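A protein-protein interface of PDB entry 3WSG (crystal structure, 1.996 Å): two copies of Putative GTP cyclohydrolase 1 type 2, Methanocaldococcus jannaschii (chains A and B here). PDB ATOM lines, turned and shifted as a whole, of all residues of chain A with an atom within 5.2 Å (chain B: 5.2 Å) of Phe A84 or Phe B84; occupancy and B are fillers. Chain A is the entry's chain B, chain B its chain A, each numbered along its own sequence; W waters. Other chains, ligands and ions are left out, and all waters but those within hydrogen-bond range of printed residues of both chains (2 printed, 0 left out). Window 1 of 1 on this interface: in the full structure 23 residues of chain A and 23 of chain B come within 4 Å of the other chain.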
ATOM      1  N   GLN A  36       3.885 -30.052   8.628  1.00  0.00           N
ATOM      2  CA  GLN A  36       4.778 -29.640   7.538  1.00  0.00           C
ATOM      3  C   GLN A  36       5.670 -28.476   8.007  1.00  0.00           C
ATOM      4  O   GLN A  36       6.896 -28.489   7.838  1.00  0.00           O
ATOM      5  CB  GLN A  36       3.963 -29.224   6.308  1.00  0.00           C
ATOM      6  CG  GLN A  36       2.862 -30.223   5.948  1.00  0.00           C
ATOM      7  CD  GLN A  36       3.429 -31.494   5.344  1.00  0.00           C
ATOM      8  OE1 GLN A  36       4.066 -31.453   4.295  1.00  0.00           O
ATOM      9  NE2 GLN A  36       3.201 -32.627   6.003  1.00  0.00           N
ATOM     10  N   VAL A  37       5.041 -27.467   8.609  1.00  0.00           N
ATOM     11  CA  VAL A  37       5.750 -26.259   9.033  1.00  0.00           C
ATOM     12  C   VAL A  37       5.158 -25.842  10.361  1.00  0.00           C
ATOM     13  O   VAL A  37       3.947 -25.667  10.469  1.00  0.00           O
ATOM     14  CB  VAL A  37       5.610 -25.111   8.004  1.00  0.00           C
ATOM     15  CG1 VAL A  37       6.303 -23.828   8.508  1.00  0.00           C
ATOM     16  CG2 VAL A  37       6.150 -25.523   6.623  1.00  0.00           C
ATOM     17  N   GLY A  38       5.992 -25.717  11.383  1.00  0.00           N
ATOM     18  CA  GLY A  38       5.500 -25.310  12.684  1.00  0.00           C
ATOM     19  C   GLY A  38       6.456 -25.692  13.793  1.00  0.00           C
ATOM     20  O   GLY A  38       7.301 -26.578  13.641  1.00  0.00           O
ATOM     21  N   LEU A  76       3.497 -30.275   1.618  1.00  0.00           N
ATOM     22  CA  LEU A  76       4.231 -29.160   1.022  1.00  0.00           C
ATOM     23  C   LEU A  76       5.321 -29.679   0.065  1.00  0.00           C
ATOM     24  O   LEU A  76       5.444 -29.207  -1.056  1.00  0.00           O
ATOM     25  CB  LEU A  76       4.844 -28.291   2.123  1.00  0.00           C
ATOM     26  CG  LEU A  76       5.641 -27.063   1.674  1.00  0.00           C
ATOM     27  CD1 LEU A  76       4.719 -26.094   0.956  1.00  0.00           C
ATOM     28  CD2 LEU A  76       6.270 -26.395   2.903  1.00  0.00           C
ATOM     29  N   LEU A  77       6.078 -30.682   0.508  1.00  0.00           N
ATOM     30  CA  LEU A  77       7.146 -31.256  -0.299  1.00  0.00           C
ATOM     31  C   LEU A  77       7.003 -32.777  -0.331  1.00  0.00           C
ATOM     32  O   LEU A  77       6.719 -33.410   0.692  1.00  0.00           O
ATOM     33  CB  LEU A  77       8.522 -30.873   0.263  1.00  0.00           C
ATOM     34  CG  LEU A  77       8.940 -29.396   0.294  1.00  0.00           C
ATOM     35  CD1 LEU A  77      10.223 -29.239   1.063  1.00  0.00           C
ATOM     36  CD2 LEU A  77       9.097 -28.810  -1.123  1.00  0.00           C
ATOM     37  N   ILE A  81      14.678 -31.190   0.383  1.00  0.00           N
ATOM     38  CA  ILE A  81      15.576 -30.170  -0.176  1.00  0.00           C
ATOM     39  C   ILE A  81      16.610 -29.743   0.861  1.00  0.00           C
ATOM     40  O   ILE A  81      16.456 -30.027   2.042  1.00  0.00           O
ATOM     41  CB  ILE A  81      14.788 -28.920  -0.644  1.00  0.00           C
ATOM     42  CG1 ILE A  81      14.063 -28.267   0.539  1.00  0.00           C
ATOM     43  CG2 ILE A  81      13.795 -29.291  -1.765  1.00  0.00           C
ATOM     44  CD1 ILE A  81      13.258 -26.987   0.177  1.00  0.00           C
ATOM     45  N   ARG A  82      17.665 -29.069   0.432  1.00  0.00           N
ATOM     46  CA  ARG A  82      18.646 -28.559   1.384  1.00  0.00           C
ATOM     47  C   ARG A  82      19.079 -27.116   1.056  1.00  0.00           C
ATOM     48  O   ARG A  82      20.118 -26.661   1.503  1.00  0.00           O
ATOM     49  CB  ARG A  82      19.857 -29.496   1.448  1.00  0.00           C
ATOM     50  CG  ARG A  82      20.497 -29.845   0.094  1.00  0.00           C
ATOM     51  CD  ARG A  82      21.644 -30.820   0.283  1.00  0.00           C
ATOM     52  NE  ARG A  82      22.601 -30.796  -0.823  1.00  0.00           N
ATOM     53  CZ  ARG A  82      23.786 -31.403  -0.807  1.00  0.00           C
ATOM     54  NH1 ARG A  82      24.183 -32.097   0.265  1.00  0.00           N
ATOM     55  NH2 ARG A  82      24.597 -31.303  -1.859  1.00  0.00           N
ATOM     56  N   ASN A  83      18.304 -26.447   0.218  1.00  0.00           N
ATOM     57  CA  ASN A  83      18.482 -25.021  -0.073  1.00  0.00           C
ATOM     58  C   ASN A  83      17.113 -24.367  -0.175  1.00  0.00           C
ATOM     59  O   ASN A  83      16.146 -25.014  -0.570  1.00  0.00           O
ATOM     60  CB  ASN A  83      19.259 -24.791  -1.372  1.00  0.00           C
ATOM     61  CG  ASN A  83      20.522 -25.620  -1.448  1.00  0.00           C
ATOM     62  OD1 ASN A  83      20.475 -26.791  -1.830  1.00  0.00           O
ATOM     63  ND2 ASN A  83      21.658 -25.032  -1.060  1.00  0.00           N
ATOM     64  N   PHE A  84      17.034 -23.083   0.152  1.00  0.00           N
ATOM     65  CA  PHE A  84      15.743 -22.424   0.302  1.00  0.00           C
ATOM     66  C   PHE A  84      15.716 -21.131  -0.473  1.00  0.00           C
ATOM     67  O   PHE A  84      16.153 -20.100   0.025  1.00  0.00           O
ATOM     68  CB  PHE A  84      15.472 -22.190   1.787  1.00  0.00           C
ATOM     69  CG  PHE A  84      15.533 -23.449   2.573  1.00  0.00           C
ATOM     70  CD1 PHE A  84      14.433 -24.292   2.623  1.00  0.00           C
ATOM     71  CD2 PHE A  84      16.708 -23.851   3.180  1.00  0.00           C
ATOM     72  CE1 PHE A  84      14.488 -25.468   3.315  1.00  0.00           C
ATOM     73  CE2 PHE A  84      16.771 -25.048   3.863  1.00  0.00           C
ATOM     74  CZ  PHE A  84      15.664 -25.858   3.928  1.00  0.00           C
ATOM     75  N   THR A  85      15.234 -21.216  -1.714  1.00  0.00           N
ATOM     76  CA  THR A  85      15.281 -20.126  -2.681  1.00  0.00           C
ATOM     77  C   THR A  85      13.994 -20.168  -3.495  1.00  0.00           C
ATOM     78  O   THR A  85      13.207 -21.109  -3.356  1.00  0.00           O
ATOM     79  CB  THR A  85      16.486 -20.256  -3.636  1.00  0.00           C
ATOM     80  OG1 THR A  85      16.281 -21.408  -4.469  1.00  0.00           O
ATOM     81  CG2 THR A  85      17.784 -20.447  -2.867  1.00  0.00           C
ATOM     82  N   GLY A  86      13.769 -19.159  -4.332  1.00  0.00           N
ATOM     83  CA  GLY A  86      12.629 -19.175  -5.237  1.00  0.00           C
ATOM     84  C   GLY A  86      11.294 -19.381  -4.528  1.00  0.00           C
ATOM     85  O   GLY A  86      11.051 -18.820  -3.451  1.00  0.00           O
ATOM     86  N   ILE A  88       9.822 -21.920  -2.875  1.00  0.00           N
ATOM     87  CA  ILE A  88       9.745 -22.503  -1.540  1.00  0.00           C
ATOM     88  C   ILE A  88      10.178 -21.457  -0.497  1.00  0.00           C
ATOM     89  O   ILE A  88       9.626 -21.416   0.595  1.00  0.00           O
ATOM     90  CB  ILE A  88      10.576 -23.808  -1.415  1.00  0.00           C
ATOM     91  CG1 ILE A  88      10.260 -24.518  -0.085  1.00  0.00           C
ATOM     92  CG2 ILE A  88      12.060 -23.567  -1.552  1.00  0.00           C
ATOM     93  CD1 ILE A  88       8.806 -25.006   0.001  1.00  0.00           C
ATOM     94  N   TYR A  89      11.121 -20.584  -0.841  1.00  0.00           N
ATOM     95  CA  TYR A  89      11.490 -19.499   0.076  1.00  0.00           C
ATOM     96  C   TYR A  89      10.281 -18.613   0.333  1.00  0.00           C
ATOM     97  O   TYR A  89       9.995 -18.258   1.479  1.00  0.00           O
ATOM     98  CB  TYR A  89      12.646 -18.655  -0.476  1.00  0.00           C
ATOM     99  CG  TYR A  89      13.059 -17.478   0.425  1.00  0.00           C
ATOM    100  CD1 TYR A  89      12.389 -16.246   0.362  1.00  0.00           C
ATOM    101  CD2 TYR A  89      14.118 -17.607   1.330  1.00  0.00           C
ATOM    102  CE1 TYR A  89      12.754 -15.168   1.187  1.00  0.00           C
ATOM    103  CE2 TYR A  89      14.508 -16.535   2.129  1.00  0.00           C
ATOM    104  CZ  TYR A  89      13.817 -15.330   2.068  1.00  0.00           C
ATOM    105  OH  TYR A  89      14.219 -14.297   2.887  1.00  0.00           O
ATOM    106  N   LEU A  92       7.658 -20.498   2.595  1.00  0.00           N
ATOM    107  CA  LEU A  92       8.117 -20.636   3.978  1.00  0.00           C
ATOM    108  C   LEU A  92       8.166 -19.280   4.685  1.00  0.00           C
ATOM    109  O   LEU A  92       7.853 -19.189   5.874  1.00  0.00           O
ATOM    110  CB  LEU A  92       9.498 -21.317   4.036  1.00  0.00           C
ATOM    111  CG  LEU A  92       9.465 -22.798   3.618  1.00  0.00           C
ATOM    112  CD1 LEU A  92      10.864 -23.383   3.579  1.00  0.00           C
ATOM    113  CD2 LEU A  92       8.576 -23.647   4.549  1.00  0.00           C
ATOM    114  N   MET A  96       6.343 -18.791   8.156  1.00  0.00           N
ATOM    115  CA  MET A  96       7.166 -18.566   9.339  1.00  0.00           C
ATOM    116  C   MET A  96       7.033 -17.179   9.897  1.00  0.00           C
ATOM    117  O   MET A  96       7.095 -17.001  11.106  1.00  0.00           O
ATOM    118  CB  MET A  96       8.633 -18.858   9.045  1.00  0.00           C
ATOM    119  CG  MET A  96       8.844 -20.356   8.861  1.00  0.00           C
ATOM    120  SD  MET A  96      10.472 -20.738   8.260  1.00  0.00           S
ATOM    121  CE  MET A  96      10.442 -22.534   8.316  1.00  0.00           C
ATOM    122  N   GLN B  36      22.383 -20.724   0.427  1.00  0.00           N
ATOM    123  CA  GLN B  36      21.669 -21.625   1.335  1.00  0.00           C
ATOM    124  C   GLN B  36      20.227 -21.166   1.521  1.00  0.00           C
ATOM    125  O   GLN B  36      19.276 -21.945   1.437  1.00  0.00           O
ATOM    126  CB  GLN B  36      22.383 -21.675   2.699  1.00  0.00           C
ATOM    127  CG  GLN B  36      23.875 -21.937   2.596  1.00  0.00           C
ATOM    128  CD  GLN B  36      24.147 -23.369   2.185  1.00  0.00           C
ATOM    129  OE1 GLN B  36      23.757 -24.295   2.890  1.00  0.00           O
ATOM    130  NE2 GLN B  36      24.829 -23.562   1.035  1.00  0.00           N
ATOM    131  N   VAL B  37      20.094 -19.878   1.815  1.00  0.00           N
ATOM    132  CA  VAL B  37      18.810 -19.264   2.069  1.00  0.00           C
ATOM    133  C   VAL B  37      18.816 -17.874   1.465  1.00  0.00           C
ATOM    134  O   VAL B  37      19.685 -17.064   1.792  1.00  0.00           O
ATOM    135  CB  VAL B  37      18.505 -19.156   3.583  1.00  0.00           C
ATOM    136  CG1 VAL B  37      17.172 -18.380   3.793  1.00  0.00           C
ATOM    137  CG2 VAL B  37      18.490 -20.552   4.241  1.00  0.00           C
ATOM    138  N   GLY B  38      17.855 -17.588   0.597  1.00  0.00           N
ATOM    139  CA  GLY B  38      17.789 -16.267  -0.004  1.00  0.00           C
ATOM    140  C   GLY B  38      16.979 -16.298  -1.273  1.00  0.00           C
ATOM    141  O   GLY B  38      16.784 -17.352  -1.881  1.00  0.00           O
ATOM    142  N   LEU B  76      24.181 -24.951   5.717  1.00  0.00           N
ATOM    143  CA  LEU B  76      23.104 -25.069   6.705  1.00  0.00           C
ATOM    144  C   LEU B  76      22.680 -26.528   6.883  1.00  0.00           C
ATOM    145  O   LEU B  76      22.524 -27.020   7.991  1.00  0.00           O
ATOM    146  CB  LEU B  76      21.904 -24.227   6.270  1.00  0.00           C
ATOM    147  CG  LEU B  76      20.671 -24.217   7.181  1.00  0.00           C
ATOM    148  CD1 LEU B  76      21.016 -23.589   8.542  1.00  0.00           C
ATOM    149  CD2 LEU B  76      19.551 -23.427   6.486  1.00  0.00           C
ATOM    150  N   LEU B  77      22.497 -27.224   5.772  1.00  0.00           N
ATOM    151  CA  LEU B  77      22.085 -28.620   5.798  1.00  0.00           C
ATOM    152  C   LEU B  77      22.999 -29.453   4.904  1.00  0.00           C
ATOM    153  O   LEU B  77      23.298 -29.050   3.779  1.00  0.00           O
ATOM    154  CB  LEU B  77      20.630 -28.739   5.320  1.00  0.00           C
ATOM    155  CG  LEU B  77      19.530 -28.071   6.152  1.00  0.00           C
ATOM    156  CD1 LEU B  77      18.187 -28.106   5.421  1.00  0.00           C
ATOM    157  CD2 LEU B  77      19.406 -28.758   7.511  1.00  0.00           C
ATOM    158  N   ILE B  81      15.782 -32.169   3.749  1.00  0.00           N
ATOM    159  CA  ILE B  81      14.609 -32.399   4.595  1.00  0.00           C
ATOM    160  C   ILE B  81      13.324 -32.012   3.868  1.00  0.00           C
ATOM    161  O   ILE B  81      13.375 -31.273   2.884  1.00  0.00           O
ATOM    162  CB  ILE B  81      14.681 -31.585   5.897  1.00  0.00           C
ATOM    163  CG1 ILE B  81      14.840 -30.102   5.566  1.00  0.00           C
ATOM    164  CG2 ILE B  81      15.869 -32.027   6.753  1.00  0.00           C
ATOM    165  CD1 ILE B  81      14.847 -29.181   6.791  1.00  0.00           C
ATOM    166  N   ARG B  82      12.174 -32.469   4.368  1.00  0.00           N
ATOM    167  CA  ARG B  82      10.885 -32.072   3.789  1.00  0.00           C
ATOM    168  C   ARG B  82       9.853 -31.684   4.863  1.00  0.00           C
ATOM    169  O   ARG B  82       8.662 -31.614   4.577  1.00  0.00           O
ATOM    170  CB  ARG B  82      10.324 -33.181   2.885  1.00  0.00           C
ATOM    171  CG  ARG B  82      10.265 -34.554   3.530  1.00  0.00           C
ATOM    172  CD  ARG B  82       9.780 -35.631   2.585  1.00  0.00           C
ATOM    173  NE  ARG B  82       9.304 -36.790   3.340  1.00  0.00           N
ATOM    174  CZ  ARG B  82       8.649 -37.823   2.822  1.00  0.00           C
ATOM    175  NH1 ARG B  82       8.354 -37.869   1.523  1.00  0.00           N
ATOM    176  NH2 ARG B  82       8.275 -38.815   3.615  1.00  0.00           N
ATOM    177  N   ASN B  83      10.319 -31.441   6.091  1.00  0.00           N
ATOM    178  CA  ASN B  83       9.482 -30.895   7.165  1.00  0.00           C
ATOM    179  C   ASN B  83      10.298 -29.846   7.915  1.00  0.00           C
ATOM    180  O   ASN B  83      11.512 -29.974   8.007  1.00  0.00           O
ATOM    181  CB  ASN B  83       9.005 -31.986   8.147  1.00  0.00           C
ATOM    182  CG  ASN B  83       8.438 -33.198   7.443  1.00  0.00           C
ATOM    183  OD1 ASN B  83       9.178 -34.095   7.056  1.00  0.00           O
ATOM    184  ND2 ASN B  83       7.134 -33.198   7.208  1.00  0.00           N
ATOM    185  N   PHE B  84       9.633 -28.825   8.464  1.00  0.00           N
ATOM    186  CA  PHE B  84      10.338 -27.652   8.991  1.00  0.00           C
ATOM    187  C   PHE B  84       9.783 -27.360  10.360  1.00  0.00           C
ATOM    188  O   PHE B  84       8.709 -26.762  10.495  1.00  0.00           O
ATOM    189  CB  PHE B  84      10.185 -26.464   8.033  1.00  0.00           C
ATOM    190  CG  PHE B  84      10.602 -26.799   6.645  1.00  0.00           C
ATOM    191  CD1 PHE B  84      11.939 -26.781   6.288  1.00  0.00           C
ATOM    192  CD2 PHE B  84       9.675 -27.237   5.721  1.00  0.00           C
ATOM    193  CE1 PHE B  84      12.331 -27.152   5.016  1.00  0.00           C
ATOM    194  CE2 PHE B  84      10.053 -27.593   4.445  1.00  0.00           C
ATOM    195  CZ  PHE B  84      11.385 -27.556   4.085  1.00  0.00           C
ATOM    196  N   THR B  85      10.472 -27.904  11.361  1.00  0.00           N
ATOM    197  CA  THR B  85      10.054 -27.900  12.759  1.00  0.00           C
ATOM    198  C   THR B  85      11.294 -27.717  13.636  1.00  0.00           C
ATOM    199  O   THR B  85      12.416 -27.752  13.131  1.00  0.00           O
ATOM    200  CB  THR B  85       9.354 -29.216  13.165  1.00  0.00           C
ATOM    201  OG1 THR B  85      10.323 -30.273  13.207  1.00  0.00           O
ATOM    202  CG2 THR B  85       8.257 -29.580  12.188  1.00  0.00           C
ATOM    203  N   GLY B  86      11.101 -27.514  14.937  1.00  0.00           N
ATOM    204  CA  GLY B  86      12.224 -27.438  15.867  1.00  0.00           C
ATOM    205  C   GLY B  86      13.293 -26.405  15.500  1.00  0.00           C
ATOM    206  O   GLY B  86      12.993 -25.273  15.107  1.00  0.00           O
ATOM    207  N   ILE B  88      15.535 -26.119  12.959  1.00  0.00           N
ATOM    208  CA  ILE B  88      15.622 -25.581  11.605  1.00  0.00           C
ATOM    209  C   ILE B  88      14.471 -24.570  11.376  1.00  0.00           C
ATOM    210  O   ILE B  88      14.639 -23.583  10.669  1.00  0.00           O
ATOM    211  CB  ILE B  88      15.618 -26.705  10.513  1.00  0.00           C
ATOM    212  CG1 ILE B  88      15.978 -26.107   9.149  1.00  0.00           C
ATOM    213  CG2 ILE B  88      14.295 -27.432  10.438  1.00  0.00           C
ATOM    214  CD1 ILE B  88      17.388 -25.546   9.111  1.00  0.00           C
ATOM    215  N   TYR B  89      13.317 -24.798  11.992  1.00  0.00           N
ATOM    216  CA  TYR B  89      12.235 -23.813  11.909  1.00  0.00           C
ATOM    217  C   TYR B  89      12.701 -22.487  12.528  1.00  0.00           C
ATOM    218  O   TYR B  89      12.511 -21.421  11.937  1.00  0.00           O
ATOM    219  CB  TYR B  89      10.960 -24.295  12.615  1.00  0.00           C
ATOM    220  CG  TYR B  89       9.835 -23.280  12.587  1.00  0.00           C
ATOM    221  CD1 TYR B  89       9.747 -22.274  13.548  1.00  0.00           C
ATOM    222  CD2 TYR B  89       8.842 -23.339  11.608  1.00  0.00           C
ATOM    223  CE1 TYR B  89       8.709 -21.340  13.522  1.00  0.00           C
ATOM    224  CE2 TYR B  89       7.807 -22.417  11.575  1.00  0.00           C
ATOM    225  CZ  TYR B  89       7.752 -21.409  12.530  1.00  0.00           C
ATOM    226  OH  TYR B  89       6.727 -20.484  12.504  1.00  0.00           O
ATOM    227  N   LEU B  92      15.391 -20.777  10.165  1.00  0.00           N
ATOM    228  CA  LEU B  92      14.837 -20.251   8.922  1.00  0.00           C
ATOM    229  C   LEU B  92      13.941 -19.036   9.216  1.00  0.00           C
ATOM    230  O   LEU B  92      13.973 -18.020   8.509  1.00  0.00           O
ATOM    231  CB  LEU B  92      14.051 -21.342   8.191  1.00  0.00           C
ATOM    232  CG  LEU B  92      14.904 -22.477   7.605  1.00  0.00           C
ATOM    233  CD1 LEU B  92      14.049 -23.572   6.976  1.00  0.00           C
ATOM    234  CD2 LEU B  92      15.868 -21.926   6.575  1.00  0.00           C
ATOM    235  N   MET B  96      14.421 -15.593   7.316  1.00  0.00           N
ATOM    236  CA  MET B  96      13.398 -15.104   6.382  1.00  0.00           C
ATOM    237  C   MET B  96      12.680 -13.860   6.838  1.00  0.00           C
ATOM    238  O   MET B  96      12.420 -12.975   6.027  1.00  0.00           O
ATOM    239  CB  MET B  96      12.392 -16.215   6.107  1.00  0.00           C
ATOM    240  CG  MET B  96      13.055 -17.303   5.298  1.00  0.00           C
ATOM    241  SD  MET B  96      12.080 -18.790   5.235  1.00  0.00           S
ATOM    242  CE  MET B  96      13.055 -19.791   4.100  1.00  0.00           C
HETATM  243  O   HOH W   1      21.631 -25.829   3.486  1.00  0.00           O
HETATM  244  O   HOH W   2       6.563 -30.886   3.337  1.00  0.00           O
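Printed residues of chain B within 4 Å of Asn A83: Gln B36.
Of the printed residues of chain B, Phe A84 touches Gln B36, Val B37, Gly B38, Leu B77, Phe B84 and Leu B92.
Of the printed residues of chain A, Ile B81 touches Ile A81.
Of chain A, only Gln A36 (2.8 Å), Val A37 (3.3 Å), Gly A38 (3.0 Å), Leu A77 (3.6 Å), Phe A84 (3.2 Å), Leu A92 (3.9 Å) and Met A96 (3.9 Å) come within 4 Å of Phe B84.
Ile B88 touches none of the printed residues of chain A.
The nearest residue of chain A that does not touch Phe B84 is Leu A76 (4.3 Å).
Water W2 lies within hydrogen-bond range of the backbone carbonyl oxygen of Arg B82 (2.5 Å), the side-chain amide oxygen of Gln A36 (2.7 Å) and the backbone NH of Leu A77 (2.9 Å).
Water W1 lies within hydrogen-bond range of the backbone carbonyl oxygen (O) of Arg A82 (2.6 Å), the side-chain amide oxygen (OE1) of Gln B36 (2.7 Å) and the backbone NH (N) of Leu B77 (2.8 Å).
Val A37 touches Phe B84, and with the chains exchanged Phe A84 touches Val B37.
Gly A38 touches Tyr B89, and with the chains exchanged Tyr A89 touches Gly B38.
Phe A84 touches its own counterpart, Phe B84.
Leu A92 touches Met B96, and with the chains exchanged Met A96 touches Leu B92.
Positions printed for both chains: 36, 37, 38, 76, 77, 81, 82, 83, 84, 85, 86, 88, 89, 92 and 96.
Of the 27 pairs that touch across the chains among the printed residues, 25 have their exchanged pair printed and touching as well.
Asn B83 touches Gln A36.
Arg B82 touches Leu A77.
CZ of Phe B84 touches CD1 of Leu A77, at 3.6 Å.
CA of Asn A83 touches O of Gln B36 (3.5 Å).
Phe A84 touches Phe B84.
CD2 of Leu B92 touches CD2 of Phe A84, at 3.99 Å.
Val B37 touches Tyr A89 (CG1 to CE2, 3.6 Å).
CG of Met B96 touches CE2 of Tyr A89 (3.6 Å).
Met A96 touches Leu B92.
Met A96 touches Met B96 (SD to SD, 3.9 Å).
Printed residues of chain B that touch a printed residue of chain A: Gln B36, Val B37, Gly B38, Leu B77, Ile B81, Arg B82, Asn B83, Phe B84, Thr B85, Tyr B89, Leu B92 and Met B96.
Of the 15 printed residues of chain A, 11 touch a printed residue of chain B.
Among the printed residues, 27 pairs touch across the chains.
Among the printed residues, no Asp or Glu carboxylate lies within 4 Å of a Lys or Arg side-chain nitrogen of the other chain.
The side-chain amide oxygen (OE1) of Gln B36 lies within hydrogen-bond range of the backbone NH (N) of Leu B76.
OE1 of Gln A36 lies within hydrogen-bond range of N of Leu A76 (3.0 Å).
The backbone NH of Gly A38 sits at hydrogen-bond distance from the backbone carbonyl oxygen of Phe B84 (3.0 Å).
N of Phe B84 lies within hydrogen-bond range of O of Gln A36 (2.8 Å).
N of Phe A84 is in hydrogen-bond range of O of Gln B36, at 2.8 Å.
The backbone carbonyl oxygen (O) of Phe A84 sits at hydrogen-bond distance from the backbone NH (N) of Gly B38 (3.1 Å).
The backbone carbonyl oxygen of Ile A81 lies within hydrogen-bond range of the backbone NH of Ile B81, 2.8 Å away.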
